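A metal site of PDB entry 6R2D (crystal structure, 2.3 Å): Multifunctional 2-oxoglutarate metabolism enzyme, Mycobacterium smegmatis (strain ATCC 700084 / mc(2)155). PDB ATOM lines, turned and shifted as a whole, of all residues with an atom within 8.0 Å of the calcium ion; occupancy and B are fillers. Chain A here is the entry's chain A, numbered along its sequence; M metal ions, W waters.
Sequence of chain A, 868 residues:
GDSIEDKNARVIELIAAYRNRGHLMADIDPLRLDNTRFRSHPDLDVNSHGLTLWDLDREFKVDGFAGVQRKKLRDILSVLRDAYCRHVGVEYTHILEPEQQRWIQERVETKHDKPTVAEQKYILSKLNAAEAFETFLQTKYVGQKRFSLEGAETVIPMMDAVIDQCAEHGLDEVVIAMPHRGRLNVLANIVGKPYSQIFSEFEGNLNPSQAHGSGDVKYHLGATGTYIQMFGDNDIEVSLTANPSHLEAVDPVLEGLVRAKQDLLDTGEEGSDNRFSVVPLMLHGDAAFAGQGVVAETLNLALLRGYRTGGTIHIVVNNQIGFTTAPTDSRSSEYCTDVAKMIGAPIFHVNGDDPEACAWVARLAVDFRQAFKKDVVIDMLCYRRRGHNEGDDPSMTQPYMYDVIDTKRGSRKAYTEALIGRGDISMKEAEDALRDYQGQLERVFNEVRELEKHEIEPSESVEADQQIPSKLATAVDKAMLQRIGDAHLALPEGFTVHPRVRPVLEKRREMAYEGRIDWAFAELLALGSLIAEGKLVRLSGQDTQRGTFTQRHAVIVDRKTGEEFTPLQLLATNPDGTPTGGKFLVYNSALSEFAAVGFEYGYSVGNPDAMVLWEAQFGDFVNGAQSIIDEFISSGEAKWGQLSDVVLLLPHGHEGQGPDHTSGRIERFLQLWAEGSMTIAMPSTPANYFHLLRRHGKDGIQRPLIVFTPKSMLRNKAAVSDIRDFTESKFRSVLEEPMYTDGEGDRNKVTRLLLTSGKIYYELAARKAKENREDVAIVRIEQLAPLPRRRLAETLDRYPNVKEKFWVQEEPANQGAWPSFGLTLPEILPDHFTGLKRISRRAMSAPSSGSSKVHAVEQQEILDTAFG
OD1 of Asp 645 sits close to N of Arg 703 (2.9 Å).
The calcium ion is bound by the backbone carbonyl oxygen (O) of Ile 701, the backbone carbonyl oxygen (O) of His 696, water W1, the side-chain carboxylate (OD1) of Asp 699, the side-chain carboxylate (OD1) of Asp 645, the side-chain carboxylate (OD2) of Asp 645 and water W2.
Water W1 lies within hydrogen-bond range of the side-chain carboxylate (OD2) of Asp 699 (2.6 Å) and a ring nitrogen (ND1) of His 696 (3.1 Å).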
ATOM      1  N   LYS A 535     -29.685  15.219  -6.162  1.00  0.00           N
ATOM      2  CA  LYS A 535     -29.168  13.869  -6.378  1.00  0.00           C
ATOM      3  C   LYS A 535     -28.743  13.176  -5.080  1.00  0.00           C
ATOM      4  O   LYS A 535     -28.141  13.801  -4.191  1.00  0.00           O
ATOM      5  CB  LYS A 535     -27.982  13.912  -7.350  1.00  0.00           C
ATOM      6  CG  LYS A 535     -27.724  12.574  -8.027  1.00  0.00           C
ATOM      7  CD  LYS A 535     -26.893  12.708  -9.260  1.00  0.00           C
ATOM      8  CE  LYS A 535     -26.758  11.383  -9.944  1.00  0.00           C
ATOM      9  NZ  LYS A 535     -27.917  11.096 -10.831  1.00  0.00           N
ATOM     10  N   PRO A 608     -30.735   3.639 -10.297  1.00  0.00           N
ATOM     11  CA  PRO A 608     -30.015   4.232 -11.451  1.00  0.00           C
ATOM     12  C   PRO A 608     -29.825   5.750 -11.340  1.00  0.00           C
ATOM     13  O   PRO A 608     -28.999   6.294 -12.059  1.00  0.00           O
ATOM     14  CB  PRO A 608     -30.938   3.904 -12.639  1.00  0.00           C
ATOM     15  CG  PRO A 608     -31.831   2.815 -12.164  1.00  0.00           C
ATOM     16  CD  PRO A 608     -32.019   3.054 -10.716  1.00  0.00           C
ATOM     17  N   ALA A 610     -28.985   7.326  -8.495  1.00  0.00           N
ATOM     18  CA  ALA A 610     -27.997   7.579  -7.455  1.00  0.00           C
ATOM     19  C   ALA A 610     -26.618   7.749  -8.046  1.00  0.00           C
ATOM     20  O   ALA A 610     -26.287   7.112  -9.054  1.00  0.00           O
ATOM     21  CB  ALA A 610     -27.981   6.429  -6.457  1.00  0.00           C
ATOM     22  N   MET A 611     -25.802   8.585  -7.389  1.00  0.00           N
ATOM     23  CA  MET A 611     -24.385   8.799  -7.689  1.00  0.00           C
ATOM     24  C   MET A 611     -23.663   7.842  -6.735  1.00  0.00           C
ATOM     25  O   MET A 611     -23.738   8.040  -5.539  1.00  0.00           O
ATOM     26  CB  MET A 611     -23.994  10.287  -7.488  1.00  0.00           C
ATOM     27  CG  MET A 611     -22.531  10.596  -7.749  1.00  0.00           C
ATOM     28  SD  MET A 611     -22.149  10.812  -9.503  1.00  0.00           S
ATOM     29  CE  MET A 611     -20.440  11.243  -9.414  1.00  0.00           C
ATOM     30  N   SER A 644     -25.253  -0.210 -15.096  1.00  0.00           N
ATOM     31  CA  SER A 644     -24.694   0.318 -13.862  1.00  0.00           C
ATOM     32  C   SER A 644     -23.919   1.585 -14.129  1.00  0.00           C
ATOM     33  O   SER A 644     -23.194   1.659 -15.102  1.00  0.00           O
ATOM     34  CB  SER A 644     -23.785  -0.709 -13.207  1.00  0.00           C
ATOM     35  OG  SER A 644     -23.057  -0.141 -12.136  1.00  0.00           O
ATOM     36  N   ASP A 645     -24.039   2.567 -13.241  1.00  0.00           N
ATOM     37  CA  ASP A 645     -23.364   3.855 -13.315  1.00  0.00           C
ATOM     38  C   ASP A 645     -22.354   3.971 -12.167  1.00  0.00           C
ATOM     39  O   ASP A 645     -21.958   5.076 -11.793  1.00  0.00           O
ATOM     40  CB  ASP A 645     -24.394   4.997 -13.268  1.00  0.00           C
ATOM     41  CG  ASP A 645     -24.054   6.232 -14.073  1.00  0.00           C
ATOM     42  OD1 ASP A 645     -23.472   6.085 -15.174  1.00  0.00           O
ATOM     43  OD2 ASP A 645     -24.389   7.347 -13.625  1.00  0.00           O
ATOM     44  N   VAL A 646     -21.914   2.828 -11.618  1.00  0.00           N
ATOM     45  CA  VAL A 646     -20.960   2.817 -10.493  1.00  0.00           C
ATOM     46  C   VAL A 646     -19.631   3.505 -10.867  1.00  0.00           C
ATOM     47  O   VAL A 646     -19.158   3.380 -11.998  1.00  0.00           O
ATOM     48  CB  VAL A 646     -20.730   1.368  -9.937  1.00  0.00           C
ATOM     49  CG1 VAL A 646     -19.952   0.470 -10.906  1.00  0.00           C
ATOM     50  CG2 VAL A 646     -20.081   1.400  -8.542  1.00  0.00           C
ATOM     51  N   VAL A 647     -19.024   4.221  -9.904  1.00  0.00           N
ATOM     52  CA  VAL A 647     -17.738   4.870 -10.058  1.00  0.00           C
ATOM     53  C   VAL A 647     -16.724   4.146  -9.195  1.00  0.00           C
ATOM     54  O   VAL A 647     -16.975   3.952  -8.006  1.00  0.00           O
ATOM     55  CB  VAL A 647     -17.765   6.398  -9.690  1.00  0.00           C
ATOM     56  CG1 VAL A 647     -16.397   7.055  -9.914  1.00  0.00           C
ATOM     57  CG2 VAL A 647     -18.876   7.139 -10.431  1.00  0.00           C
ATOM     58  N   THR A 679     -16.239   4.212 -19.017  1.00  0.00           N
ATOM     59  CA  THR A 679     -15.488   5.445 -19.198  1.00  0.00           C
ATOM     60  C   THR A 679     -14.272   5.288 -18.296  1.00  0.00           C
ATOM     61  O   THR A 679     -14.429   4.898 -17.137  1.00  0.00           O
ATOM     62  CB  THR A 679     -16.320   6.700 -18.903  1.00  0.00           C
ATOM     63  OG1 THR A 679     -17.550   6.630 -19.616  1.00  0.00           O
ATOM     64  CG2 THR A 679     -15.573   7.996 -19.269  1.00  0.00           C
ATOM     65  N   LEU A 692     -15.735  15.923 -14.642  1.00  0.00           N
ATOM     66  CA  LEU A 692     -15.849  14.481 -14.938  1.00  0.00           C
ATOM     67  C   LEU A 692     -16.962  13.835 -14.073  1.00  0.00           C
ATOM     68  O   LEU A 692     -17.774  13.083 -14.607  1.00  0.00           O
ATOM     69  CB  LEU A 692     -14.492  13.769 -14.683  1.00  0.00           C
ATOM     70  CG  LEU A 692     -14.448  12.250 -14.942  1.00  0.00           C
ATOM     71  CD1 LEU A 692     -14.289  11.933 -16.448  1.00  0.00           C
ATOM     72  CD2 LEU A 692     -13.360  11.591 -14.114  1.00  0.00           C
ATOM     73  N   LEU A 693     -16.991  14.143 -12.746  1.00  0.00           N
ATOM     74  CA  LEU A 693     -17.993  13.613 -11.804  1.00  0.00           C
ATOM     75  C   LEU A 693     -19.388  14.174 -12.080  1.00  0.00           C
ATOM     76  O   LEU A 693     -20.379  13.432 -12.022  1.00  0.00           O
ATOM     77  CB  LEU A 693     -17.611  13.883 -10.335  1.00  0.00           C
ATOM     78  CG  LEU A 693     -16.346  13.172  -9.787  1.00  0.00           C
ATOM     79  CD1 LEU A 693     -16.106  13.549  -8.333  1.00  0.00           C
ATOM     80  CD2 LEU A 693     -16.436  11.646  -9.920  1.00  0.00           C
ATOM     81  N   ARG A 694     -19.475  15.484 -12.381  1.00  0.00           N
ATOM     82  CA  ARG A 694     -20.767  16.116 -12.680  1.00  0.00           C
ATOM     83  C   ARG A 694     -21.307  15.623 -14.036  1.00  0.00           C
ATOM     84  O   ARG A 694     -22.506  15.357 -14.122  1.00  0.00           O
ATOM     85  CB  ARG A 694     -20.671  17.645 -12.613  1.00  0.00           C
ATOM     86  CG  ARG A 694     -20.754  18.095 -11.166  1.00  0.00           C
ATOM     87  CD  ARG A 694     -20.755  19.593 -11.003  1.00  0.00           C
ATOM     88  NE  ARG A 694     -21.826  20.264 -11.746  1.00  0.00           N
ATOM     89  CZ  ARG A 694     -23.099  20.298 -11.377  1.00  0.00           C
ATOM     90  NH1 ARG A 694     -23.501  19.689 -10.275  1.00  0.00           N
ATOM     91  NH2 ARG A 694     -23.990  20.950 -12.108  1.00  0.00           N
ATOM     92  N   ARG A 695     -20.431  15.434 -15.058  1.00  0.00           N
ATOM     93  CA  ARG A 695     -20.881  14.888 -16.364  1.00  0.00           C
ATOM     94  C   ARG A 695     -21.438  13.498 -16.130  1.00  0.00           C
ATOM     95  O   ARG A 695     -22.557  13.231 -16.559  1.00  0.00           O
ATOM     96  CB  ARG A 695     -19.746  14.872 -17.424  1.00  0.00           C
ATOM     97  CG  ARG A 695     -20.153  14.263 -18.781  1.00  0.00           C
ATOM     98  CD  ARG A 695     -19.035  14.156 -19.792  1.00  0.00           C
ATOM     99  NE  ARG A 695     -18.029  13.149 -19.427  1.00  0.00           N
ATOM    100  CZ  ARG A 695     -17.014  12.760 -20.202  1.00  0.00           C
ATOM    101  NH1 ARG A 695     -16.840  13.292 -21.408  1.00  0.00           N
ATOM    102  NH2 ARG A 695     -16.156  11.854 -19.763  1.00  0.00           N
ATOM    103  N   HIS A 696     -20.718  12.652 -15.376  1.00  0.00           N
ATOM    104  CA  HIS A 696     -21.113  11.285 -15.063  1.00  0.00           C
ATOM    105  C   HIS A 696     -22.479  11.201 -14.379  1.00  0.00           C
ATOM    106  O   HIS A 696     -23.281  10.336 -14.717  1.00  0.00           O
ATOM    107  CB  HIS A 696     -20.077  10.596 -14.191  1.00  0.00           C
ATOM    108  CG  HIS A 696     -20.381   9.164 -13.945  1.00  0.00           C
ATOM    109  ND1 HIS A 696     -20.267   8.216 -14.936  1.00  0.00           N
ATOM    110  CD2 HIS A 696     -20.861   8.567 -12.824  1.00  0.00           C
ATOM    111  CE1 HIS A 696     -20.625   7.072 -14.383  1.00  0.00           C
ATOM    112  NE2 HIS A 696     -20.991   7.227 -13.125  1.00  0.00           N
ATOM    113  N   GLY A 697     -22.727  12.088 -13.413  1.00  0.00           N
ATOM    114  CA  GLY A 697     -23.980  12.102 -12.666  1.00  0.00           C
ATOM    115  C   GLY A 697     -25.148  12.724 -13.383  1.00  0.00           C
ATOM    116  O   GLY A 697     -26.294  12.453 -13.023  1.00  0.00           O
ATOM    117  N   LYS A 698     -24.907  13.575 -14.398  1.00  0.00           N
ATOM    118  CA  LYS A 698     -25.978  14.305 -15.093  1.00  0.00           C
ATOM    119  C   LYS A 698     -26.179  13.917 -16.579  1.00  0.00           C
ATOM    120  O   LYS A 698     -27.130  14.418 -17.180  1.00  0.00           O
ATOM    121  CB  LYS A 698     -25.696  15.820 -15.024  1.00  0.00           C
ATOM    122  CG  LYS A 698     -25.590  16.408 -13.610  1.00  0.00           C
ATOM    123  CD  LYS A 698     -24.963  17.817 -13.596  1.00  0.00           C
ATOM    124  CE  LYS A 698     -25.880  18.906 -14.145  1.00  0.00           C
ATOM    125  NZ  LYS A 698     -27.108  19.053 -13.323  1.00  0.00           N
ATOM    126  N   ASP A 699     -25.315  13.058 -17.169  1.00  0.00           N
ATOM    127  CA  ASP A 699     -25.373  12.686 -18.590  1.00  0.00           C
ATOM    128  C   ASP A 699     -26.561  11.791 -18.987  1.00  0.00           C
ATOM    129  O   ASP A 699     -26.781  11.599 -20.173  1.00  0.00           O
ATOM    130  CB  ASP A 699     -24.055  12.001 -19.033  1.00  0.00           C
ATOM    131  CG  ASP A 699     -23.685  10.732 -18.289  1.00  0.00           C
ATOM    132  OD1 ASP A 699     -24.517  10.222 -17.499  1.00  0.00           O
ATOM    133  OD2 ASP A 699     -22.554  10.234 -18.509  1.00  0.00           O
ATOM    134  N   GLY A 700     -27.262  11.225 -18.002  1.00  0.00           N
ATOM    135  CA  GLY A 700     -28.413  10.351 -18.247  1.00  0.00           C
ATOM    136  C   GLY A 700     -28.063   9.005 -18.864  1.00  0.00           C
ATOM    137  O   GLY A 700     -28.935   8.336 -19.418  1.00  0.00           O
ATOM    138  N   ILE A 701     -26.772   8.623 -18.796  1.00  0.00           N
ATOM    139  CA  ILE A 701     -26.188   7.399 -19.339  1.00  0.00           C
ATOM    140  C   ILE A 701     -25.792   6.507 -18.170  1.00  0.00           C
ATOM    141  O   ILE A 701     -25.168   7.009 -17.231  1.00  0.00           O
ATOM    142  CB  ILE A 701     -24.975   7.758 -20.258  1.00  0.00           C
ATOM    143  CG1 ILE A 701     -25.438   8.495 -21.535  1.00  0.00           C
ATOM    144  CG2 ILE A 701     -24.124   6.526 -20.619  1.00  0.00           C
ATOM    145  CD1 ILE A 701     -24.439   9.508 -22.089  1.00  0.00           C
ATOM    146  N   GLN A 702     -26.172   5.211 -18.202  1.00  0.00           N
ATOM    147  CA  GLN A 702     -25.800   4.292 -17.129  1.00  0.00           C
ATOM    148  C   GLN A 702     -24.587   3.504 -17.614  1.00  0.00           C
ATOM    149  O   GLN A 702     -24.720   2.512 -18.343  1.00  0.00           O
ATOM    150  CB  GLN A 702     -26.977   3.402 -16.701  1.00  0.00           C
ATOM    151  CG  GLN A 702     -28.244   4.128 -16.238  1.00  0.00           C
ATOM    152  CD  GLN A 702     -28.016   5.005 -15.047  1.00  0.00           C
ATOM    153  OE1 GLN A 702     -27.586   4.552 -13.989  1.00  0.00           O
ATOM    154  NE2 GLN A 702     -28.282   6.295 -15.192  1.00  0.00           N
ATOM    155  N   ARG A 703     -23.378   3.995 -17.251  1.00  0.00           N
ATOM    156  CA  ARG A 703     -22.106   3.399 -17.660  1.00  0.00           C
ATOM    157  C   ARG A 703     -21.071   3.551 -16.544  1.00  0.00           C
ATOM    158  O   ARG A 703     -20.865   4.654 -16.049  1.00  0.00           O
ATOM    159  CB  ARG A 703     -21.627   4.099 -18.949  1.00  0.00           C
ATOM    160  CG  ARG A 703     -20.446   3.442 -19.661  1.00  0.00           C
ATOM    161  CD  ARG A 703     -20.263   3.951 -21.088  1.00  0.00           C
ATOM    162  NE  ARG A 703     -21.512   3.832 -21.850  1.00  0.00           N
ATOM    163  CZ  ARG A 703     -21.742   4.369 -23.041  1.00  0.00           C
ATOM    164  NH1 ARG A 703     -20.793   5.051 -23.668  1.00  0.00           N
ATOM    165  NH2 ARG A 703     -22.925   4.222 -23.618  1.00  0.00           N
ATOM    166  N   PRO A 704     -20.342   2.482 -16.177  1.00  0.00           N
ATOM    167  CA  PRO A 704     -19.337   2.643 -15.110  1.00  0.00           C
ATOM    168  C   PRO A 704     -18.221   3.601 -15.478  1.00  0.00           C
ATOM    169  O   PRO A 704     -17.848   3.728 -16.638  1.00  0.00           O
ATOM    170  CB  PRO A 704     -18.817   1.217 -14.912  1.00  0.00           C
ATOM    171  CG  PRO A 704     -19.929   0.334 -15.440  1.00  0.00           C
ATOM    172  CD  PRO A 704     -20.418   1.075 -16.628  1.00  0.00           C
ATOM    173  N   LEU A 705     -17.702   4.308 -14.458  1.00  0.00           N
ATOM    174  CA  LEU A 705     -16.619   5.257 -14.597  1.00  0.00           C
ATOM    175  C   LEU A 705     -15.460   4.776 -13.735  1.00  0.00           C
ATOM    176  O   LEU A 705     -15.627   4.551 -12.542  1.00  0.00           O
ATOM    177  CB  LEU A 705     -17.072   6.670 -14.214  1.00  0.00           C
ATOM    178  CG  LEU A 705     -16.005   7.801 -14.092  1.00  0.00           C
ATOM    179  CD1 LEU A 705     -15.393   8.179 -15.446  1.00  0.00           C
ATOM    180  CD2 LEU A 705     -16.612   9.045 -13.485  1.00  0.00           C
HETATM  181 CA    CA M   1     -24.034   8.428 -15.879  1.00  0.00          CA
HETATM  182  O   HOH W   1     -22.240   7.900 -17.314  1.00  0.00           O
HETATM  183  O   HOH W   2     -26.295   9.060 -14.888  1.00  0.00           O
